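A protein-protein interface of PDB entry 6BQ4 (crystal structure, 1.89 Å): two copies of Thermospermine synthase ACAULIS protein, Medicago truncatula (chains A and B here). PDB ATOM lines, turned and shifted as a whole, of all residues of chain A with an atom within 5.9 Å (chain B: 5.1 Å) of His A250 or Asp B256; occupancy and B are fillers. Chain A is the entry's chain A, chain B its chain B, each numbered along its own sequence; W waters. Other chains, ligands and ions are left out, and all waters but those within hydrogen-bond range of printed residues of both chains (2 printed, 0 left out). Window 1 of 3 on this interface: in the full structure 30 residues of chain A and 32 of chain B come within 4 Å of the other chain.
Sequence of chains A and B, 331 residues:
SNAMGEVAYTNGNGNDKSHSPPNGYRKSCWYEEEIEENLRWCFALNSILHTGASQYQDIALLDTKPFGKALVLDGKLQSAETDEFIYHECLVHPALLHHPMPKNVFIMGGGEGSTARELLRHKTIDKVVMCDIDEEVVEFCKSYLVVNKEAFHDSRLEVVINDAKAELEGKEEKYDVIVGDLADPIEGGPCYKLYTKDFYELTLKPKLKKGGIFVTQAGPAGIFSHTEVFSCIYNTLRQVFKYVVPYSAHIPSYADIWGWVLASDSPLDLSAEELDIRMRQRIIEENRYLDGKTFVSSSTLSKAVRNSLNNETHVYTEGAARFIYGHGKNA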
ATOM      1  N   ILE A  86      12.130  16.975  36.127  1.00  0.00           N
ATOM      2  CA  ILE A  86      11.093  16.201  35.496  1.00  0.00           C
ATOM      3  C   ILE A  86      10.296  15.532  36.614  1.00  0.00           C
ATOM      4  O   ILE A  86       9.059  15.661  36.690  1.00  0.00           O
ATOM      5  CB  ILE A  86      11.622  15.149  34.510  1.00  0.00           C
ATOM      6  CG1 ILE A  86      12.428  15.797  33.403  1.00  0.00           C
ATOM      7  CG2 ILE A  86      10.457  14.396  33.875  1.00  0.00           C
ATOM      8  CD1 ILE A  86      13.032  14.743  32.499  1.00  0.00           C
ATOM      9  N   SER A 248       2.699   8.962  34.008  1.00  0.00           N
ATOM     10  CA  SER A 248       4.065   8.519  33.962  1.00  0.00           C
ATOM     11  C   SER A 248       4.902   9.378  33.013  1.00  0.00           C
ATOM     12  O   SER A 248       4.362  10.066  32.149  1.00  0.00           O
ATOM     13  CB  SER A 248       4.064   7.027  33.590  1.00  0.00           C
ATOM     14  OG  SER A 248       3.684   6.838  32.246  1.00  0.00           O
ATOM     15  N   ALA A 249       6.210   9.386  33.229  1.00  0.00           N
ATOM     16  CA  ALA A 249       7.144  10.101  32.390  1.00  0.00           C
ATOM     17  C   ALA A 249       8.525   9.455  32.504  1.00  0.00           C
ATOM     18  O   ALA A 249       8.911   8.933  33.530  1.00  0.00           O
ATOM     19  CB  ALA A 249       7.229  11.573  32.788  1.00  0.00           C
ATOM     20  N   HIS A 250       9.276   9.532  31.410  1.00  0.00           N
ATOM     21  CA  HIS A 250      10.639   9.081  31.364  1.00  0.00           C
ATOM     22  C   HIS A 250      11.526   9.995  32.222  1.00  0.00           C
ATOM     23  O   HIS A 250      11.448  11.211  32.134  1.00  0.00           O
ATOM     24  CB  HIS A 250      11.128   9.089  29.936  1.00  0.00           C
ATOM     25  CG  HIS A 250      12.531   8.581  29.771  1.00  0.00           C
ATOM     26  ND1 HIS A 250      13.523   9.314  29.161  1.00  0.00           N
ATOM     27  CD2 HIS A 250      13.098   7.412  30.132  1.00  0.00           C
ATOM     28  CE1 HIS A 250      14.637   8.615  29.158  1.00  0.00           C
ATOM     29  NE2 HIS A 250      14.408   7.459  29.746  1.00  0.00           N
ATOM     30  N   ILE A 251      12.370   9.372  33.033  1.00  0.00           N
ATOM     31  CA  ILE A 251      13.413  10.060  33.765  1.00  0.00           C
ATOM     32  C   ILE A 251      14.750   9.506  33.284  1.00  0.00           C
ATOM     33  O   ILE A 251      15.110   8.407  33.626  1.00  0.00           O
ATOM     34  CB  ILE A 251      13.217   9.920  35.267  1.00  0.00           C
ATOM     35  CG1 ILE A 251      11.886  10.595  35.673  1.00  0.00           C
ATOM     36  CG2 ILE A 251      14.373  10.614  35.995  1.00  0.00           C
ATOM     37  CD1 ILE A 251      11.526  10.390  37.104  1.00  0.00           C
ATOM     38  N   PRO A 252      15.516  10.291  32.495  1.00  0.00           N
ATOM     39  CA  PRO A 252      16.724   9.772  31.846  1.00  0.00           C
ATOM     40  C   PRO A 252      17.713   9.077  32.780  1.00  0.00           C
ATOM     41  O   PRO A 252      18.210   8.007  32.439  1.00  0.00           O
ATOM     42  CB  PRO A 252      17.364  11.031  31.206  1.00  0.00           C
ATOM     43  CG  PRO A 252      16.190  11.878  30.890  1.00  0.00           C
ATOM     44  CD  PRO A 252      15.163  11.630  31.992  1.00  0.00           C
ATOM     45  N   ALA A 255      16.923   5.601  33.860  1.00  0.00           N
ATOM     46  CA  ALA A 255      16.744   4.659  32.745  1.00  0.00           C
ATOM     47  C   ALA A 255      15.421   3.873  32.785  1.00  0.00           C
ATOM     48  O   ALA A 255      15.310   2.714  32.299  1.00  0.00           O
ATOM     49  CB  ALA A 255      17.946   3.712  32.605  1.00  0.00           C
ATOM     50  N   ASP A 256      14.382   4.552  33.243  1.00  0.00           N
ATOM     51  CA  ASP A 256      13.064   3.956  33.190  1.00  0.00           C
ATOM     52  C   ASP A 256      12.059   5.070  33.078  1.00  0.00           C
ATOM     53  O   ASP A 256      12.386   6.231  33.260  1.00  0.00           O
ATOM     54  CB  ASP A 256      12.836   3.106  34.448  1.00  0.00           C
ATOM     55  CG  ASP A 256      11.907   1.948  34.234  1.00  0.00           C
ATOM     56  OD1 ASP A 256      11.255   1.853  33.139  1.00  0.00           O
ATOM     57  OD2 ASP A 256      11.777   1.135  35.186  1.00  0.00           O
ATOM     58  N   ILE A 257      10.841   4.671  32.772  1.00  0.00           N
ATOM     59  CA  ILE A 257       9.659   5.474  32.958  1.00  0.00           C
ATOM     60  C   ILE A 257       9.333   5.401  34.484  1.00  0.00           C
ATOM     61  O   ILE A 257       9.444   4.330  35.084  1.00  0.00           O
ATOM     62  CB  ILE A 257       8.478   4.904  32.177  1.00  0.00           C
ATOM     63  CG1 ILE A 257       8.767   4.823  30.681  1.00  0.00           C
ATOM     64  CG2 ILE A 257       7.236   5.744  32.424  1.00  0.00           C
ATOM     65  CD1 ILE A 257       9.239   6.094  30.036  1.00  0.00           C
ATOM     66  N   TRP A 258       8.886   6.505  35.066  1.00  0.00           N
ATOM     67  CA  TRP A 258       8.484   6.561  36.481  1.00  0.00           C
ATOM     68  C   TRP A 258       7.017   6.994  36.552  1.00  0.00           C
ATOM     69  O   TRP A 258       6.515   7.671  35.648  1.00  0.00           O
ATOM     70  CB  TRP A 258       9.410   7.580  37.244  1.00  0.00           C
ATOM     71  CG  TRP A 258       9.543   7.213  38.644  1.00  0.00           C
ATOM     72  CD1 TRP A 258       8.880   7.747  39.702  1.00  0.00           C
ATOM     73  CD2 TRP A 258      10.302   6.127  39.146  1.00  0.00           C
ATOM     74  NE1 TRP A 258       9.217   7.085  40.872  1.00  0.00           N
ATOM     75  CE2 TRP A 258      10.116   6.107  40.562  1.00  0.00           C
ATOM     76  CE3 TRP A 258      11.156   5.183  38.555  1.00  0.00           C
ATOM     77  CZ2 TRP A 258      10.739   5.180  41.374  1.00  0.00           C
ATOM     78  CZ3 TRP A 258      11.804   4.270  39.374  1.00  0.00           C
ATOM     79  CH2 TRP A 258      11.579   4.270  40.776  1.00  0.00           C
ATOM     80  N   TYR A 289       9.334  21.198  32.190  1.00  0.00           N
ATOM     81  CA  TYR A 289       8.946  19.904  31.599  1.00  0.00           C
ATOM     82  C   TYR A 289       7.474  19.870  31.199  1.00  0.00           C
ATOM     83  O   TYR A 289       7.116  19.537  30.076  1.00  0.00           O
ATOM     84  CB  TYR A 289       9.260  18.723  32.531  1.00  0.00           C
ATOM     85  CG  TYR A 289       8.779  17.402  31.953  1.00  0.00           C
ATOM     86  CD1 TYR A 289       9.415  16.847  30.834  1.00  0.00           C
ATOM     87  CD2 TYR A 289       7.643  16.780  32.449  1.00  0.00           C
ATOM     88  CE1 TYR A 289       8.961  15.668  30.254  1.00  0.00           C
ATOM     89  CE2 TYR A 289       7.170  15.605  31.884  1.00  0.00           C
ATOM     90  CZ  TYR A 289       7.824  15.051  30.791  1.00  0.00           C
ATOM     91  OH  TYR A 289       7.349  13.889  30.244  1.00  0.00           O
ATOM     92  N   PRO B 220      17.197   8.791  18.768  1.00  0.00           N
ATOM     93  CA  PRO B 220      16.743   8.992  20.153  1.00  0.00           C
ATOM     94  C   PRO B 220      15.756  10.196  20.239  1.00  0.00           C
ATOM     95  O   PRO B 220      15.842  11.155  19.440  1.00  0.00           O
ATOM     96  CB  PRO B 220      18.027   9.331  20.896  1.00  0.00           C
ATOM     97  CG  PRO B 220      19.165   9.082  19.942  1.00  0.00           C
ATOM     98  CD  PRO B 220      18.632   9.074  18.561  1.00  0.00           C
ATOM     99  N   ALA B 221      14.866  10.172  21.209  1.00  0.00           N
ATOM    100  CA  ALA B 221      13.865  11.209  21.330  1.00  0.00           C
ATOM    101  C   ALA B 221      13.649  11.550  22.790  1.00  0.00           C
ATOM    102  O   ALA B 221      12.562  11.905  23.193  1.00  0.00           O
ATOM    103  CB  ALA B 221      12.558  10.748  20.673  1.00  0.00           C
ATOM    104  N   GLY B 222      14.693  11.414  23.581  1.00  0.00           N
ATOM    105  CA  GLY B 222      14.606  11.744  25.003  1.00  0.00           C
ATOM    106  C   GLY B 222      14.638  13.244  25.173  1.00  0.00           C
ATOM    107  O   GLY B 222      14.954  14.020  24.232  1.00  0.00           O
ATOM    108  N   SER B 225      18.194  13.947  24.439  1.00  0.00           N
ATOM    109  CA  SER B 225      18.773  13.328  23.245  1.00  0.00           C
ATOM    110  C   SER B 225      18.014  13.620  21.956  1.00  0.00           C
ATOM    111  O   SER B 225      18.555  13.348  20.852  1.00  0.00           O
ATOM    112  CB  SER B 225      18.868  11.852  23.459  1.00  0.00           C
ATOM    113  OG  SER B 225      17.577  11.314  23.629  1.00  0.00           O
ATOM    114  N   ALA B 249       8.431   6.603  21.816  1.00  0.00           N
ATOM    115  CA  ALA B 249       8.151   5.640  22.851  1.00  0.00           C
ATOM    116  C   ALA B 249       9.431   5.120  23.500  1.00  0.00           C
ATOM    117  O   ALA B 249      10.494   5.020  22.875  1.00  0.00           O
ATOM    118  CB  ALA B 249       7.414   4.454  22.243  1.00  0.00           C
ATOM    119  N   HIS B 250       9.312   4.728  24.766  1.00  0.00           N
ATOM    120  CA  HIS B 250      10.423   4.174  25.523  1.00  0.00           C
ATOM    121  C   HIS B 250      10.742   2.746  25.053  1.00  0.00           C
ATOM    122  O   HIS B 250       9.829   1.955  24.844  1.00  0.00           O
ATOM    123  CB  HIS B 250      10.021   4.086  26.991  1.00  0.00           C
ATOM    124  CG  HIS B 250      11.113   3.563  27.874  1.00  0.00           C
ATOM    125  ND1 HIS B 250      10.902   2.575  28.803  1.00  0.00           N
ATOM    126  CD2 HIS B 250      12.416   3.891  27.958  1.00  0.00           C
ATOM    127  CE1 HIS B 250      12.036   2.316  29.415  1.00  0.00           C
ATOM    128  NE2 HIS B 250      12.965   3.112  28.932  1.00  0.00           N
ATOM    129  N   ILE B 251      12.032   2.442  24.860  1.00  0.00           N
ATOM    130  CA  ILE B 251      12.470   1.108  24.552  1.00  0.00           C
ATOM    131  C   ILE B 251      13.481   0.741  25.647  1.00  0.00           C
ATOM    132  O   ILE B 251      14.574   1.332  25.690  1.00  0.00           O
ATOM    133  CB  ILE B 251      13.099   1.030  23.148  1.00  0.00           C
ATOM    134  CG1 ILE B 251      12.021   1.330  22.110  1.00  0.00           C
ATOM    135  CG2 ILE B 251      13.622  -0.355  22.871  1.00  0.00           C
ATOM    136  CD1 ILE B 251      12.636   1.770  20.853  1.00  0.00           C
ATOM    137  N   TYR B 254      17.100   0.107  24.973  1.00  0.00           N
ATOM    138  CA  TYR B 254      17.920   1.168  24.376  1.00  0.00           C
ATOM    139  C   TYR B 254      18.275   2.204  25.412  1.00  0.00           C
ATOM    140  O   TYR B 254      18.929   3.175  25.077  1.00  0.00           O
ATOM    141  CB  TYR B 254      17.204   1.899  23.266  1.00  0.00           C
ATOM    142  CG  TYR B 254      16.907   1.179  21.969  1.00  0.00           C
ATOM    143  CD1 TYR B 254      17.095  -0.196  21.792  1.00  0.00           C
ATOM    144  CD2 TYR B 254      16.454   1.899  20.909  1.00  0.00           C
ATOM    145  CE1 TYR B 254      16.808  -0.814  20.570  1.00  0.00           C
ATOM    146  CE2 TYR B 254      16.159   1.321  19.707  1.00  0.00           C
ATOM    147  CZ  TYR B 254      16.327  -0.032  19.520  1.00  0.00           C
ATOM    148  OH  TYR B 254      15.957  -0.565  18.293  1.00  0.00           O
ATOM    149  N   ALA B 255      17.797   2.065  26.636  1.00  0.00           N
ATOM    150  CA  ALA B 255      18.018   3.092  27.657  1.00  0.00           C
ATOM    151  C   ALA B 255      17.560   4.574  27.299  1.00  0.00           C
ATOM    152  O   ALA B 255      18.067   5.580  27.861  1.00  0.00           O
ATOM    153  CB  ALA B 255      19.482   3.043  28.040  1.00  0.00           C
ATOM    154  N   ASP B 256      16.546   4.690  26.434  1.00  0.00           N
ATOM    155  CA  ASP B 256      16.077   5.973  25.966  1.00  0.00           C
ATOM    156  C   ASP B 256      14.713   5.825  25.301  1.00  0.00           C
ATOM    157  O   ASP B 256      14.229   4.713  25.009  1.00  0.00           O
ATOM    158  CB  ASP B 256      17.102   6.597  24.975  1.00  0.00           C
ATOM    159  CG  ASP B 256      17.114   8.145  24.956  1.00  0.00           C
ATOM    160  OD1 ASP B 256      16.245   8.763  25.600  1.00  0.00           O
ATOM    161  OD2 ASP B 256      17.967   8.734  24.220  1.00  0.00           O
ATOM    162  N   ILE B 257      14.125   6.971  25.057  1.00  0.00           N
ATOM    163  CA  ILE B 257      12.944   7.117  24.288  1.00  0.00           C
ATOM    164  C   ILE B 257      13.462   7.133  22.866  1.00  0.00           C
ATOM    165  O   ILE B 257      14.505   7.809  22.584  1.00  0.00           O
ATOM    166  CB  ILE B 257      12.241   8.450  24.597  1.00  0.00           C
ATOM    167  CG1 ILE B 257      11.795   8.568  26.079  1.00  0.00           C
ATOM    168  CG2 ILE B 257      11.055   8.615  23.703  1.00  0.00           C
ATOM    169  CD1 ILE B 257      10.973   7.427  26.568  1.00  0.00           C
ATOM    170  N   TRP B 258      12.773   6.396  22.012  1.00  0.00           N
ATOM    171  CA  TRP B 258      13.057   6.361  20.577  1.00  0.00           C
ATOM    172  C   TRP B 258      12.011   7.104  19.753  1.00  0.00           C
ATOM    173  O   TRP B 258      10.855   7.207  20.137  1.00  0.00           O
ATOM    174  CB  TRP B 258      13.238   4.911  20.081  1.00  0.00           C
ATOM    175  CG  TRP B 258      14.268   4.881  18.964  1.00  0.00           C
ATOM    176  CD1 TRP B 258      14.039   4.719  17.627  1.00  0.00           C
ATOM    177  CD2 TRP B 258      15.654   5.051  19.121  1.00  0.00           C
ATOM    178  NE1 TRP B 258      15.232   4.812  16.917  1.00  0.00           N
ATOM    179  CE2 TRP B 258      16.241   5.003  17.825  1.00  0.00           C
ATOM    180  CE3 TRP B 258      16.471   5.293  20.226  1.00  0.00           C
ATOM    181  CZ2 TRP B 258      17.600   5.199  17.623  1.00  0.00           C
ATOM    182  CZ3 TRP B 258      17.813   5.483  20.031  1.00  0.00           C
ATOM    183  CH2 TRP B 258      18.377   5.449  18.736  1.00  0.00           C
HETATM  184  O   HOH W   1      17.378   6.730  30.187  1.00  0.00           O
HETATM  185  O   HOH W   2      15.499   2.088  29.747  1.00  0.00           O
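Water W2 bridges the backbone carbonyl oxygen (O) of Ala A255 (2.6 Å) and a ring nitrogen (NE2) of His B250 (2.9 Å). Water W1 lies within hydrogen-bond range of O of Ala B255 (2.7 Å), O of Pro A252 (2.7 Å) and NE2 of His A250 (3.1 Å).
His A250 touches Asp B256 (CE1 to OD1, 3.9 Å). CG1 of Ile B257 touches ND1 of His A250, 3.6 Å away. OD1 of Asp A256 touches CE1 of His B250, 3.8 Å away. His B250 touches Ile A257 (ND1 to CG1, 3.6 Å).
The backbone NH (N) of Ile A251 is in hydrogen-bond range of the backbone carbonyl oxygen (O) of Asp A256, 3.1 Å away. The backbone NH (N) of Ala B221 is in hydrogen-bond range of the backbone carbonyl oxygen (O) of Ile B257 (2.8 Å). The side-chain hydroxyl (OG) of Ser B225 is in hydrogen-bond range of the side-chain carboxylate (OD2) of Asp B256, at 2.7 Å. N of Ile B251 sits at hydrogen-bond distance from O of Asp B256, 3.2 Å away.
Ala A249 touches none of the printed residues of chain B. His A250 touches just these residues of chain B: Asp B256 and Ile B257. Ile A251 touches none of the printed residues of chain B. Of the printed residues of chain B, Asp A256 touches His B250. Of the printed residues of chain B, Ile A257 touches His B250. Printed residues of chain A within 4 Å of His B250: Asp A256 and Ile A257. Printed residues of chain A within 4 Å of Asp B256: His A250. Of the printed residues of chain A, Ile B257 touches His A250 (3.6 Å).
Of the 11 printed residues of chain A, 3 touch a printed residue of chain B. Printed residues of chain A that touch a printed residue of chain B: His A250, Asp A256 and Ile A257. Hydrophobic or aromatic side chains of chain A within 4 Å of the printed part of chain B: His A250 and Ile A257.
His A250 touches Asp B256, and with the chains exchanged Asp A256 touches His B250. His A250 touches Ile B257, and with the chains exchanged Ile A257 touches His B250. Positions printed for both chains: 249, 250, 251, 255, 256, 257 and 258. Of the 4 pairs that touch across the chains among the printed residues, 4 have their exchanged pair printed and touching as well.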
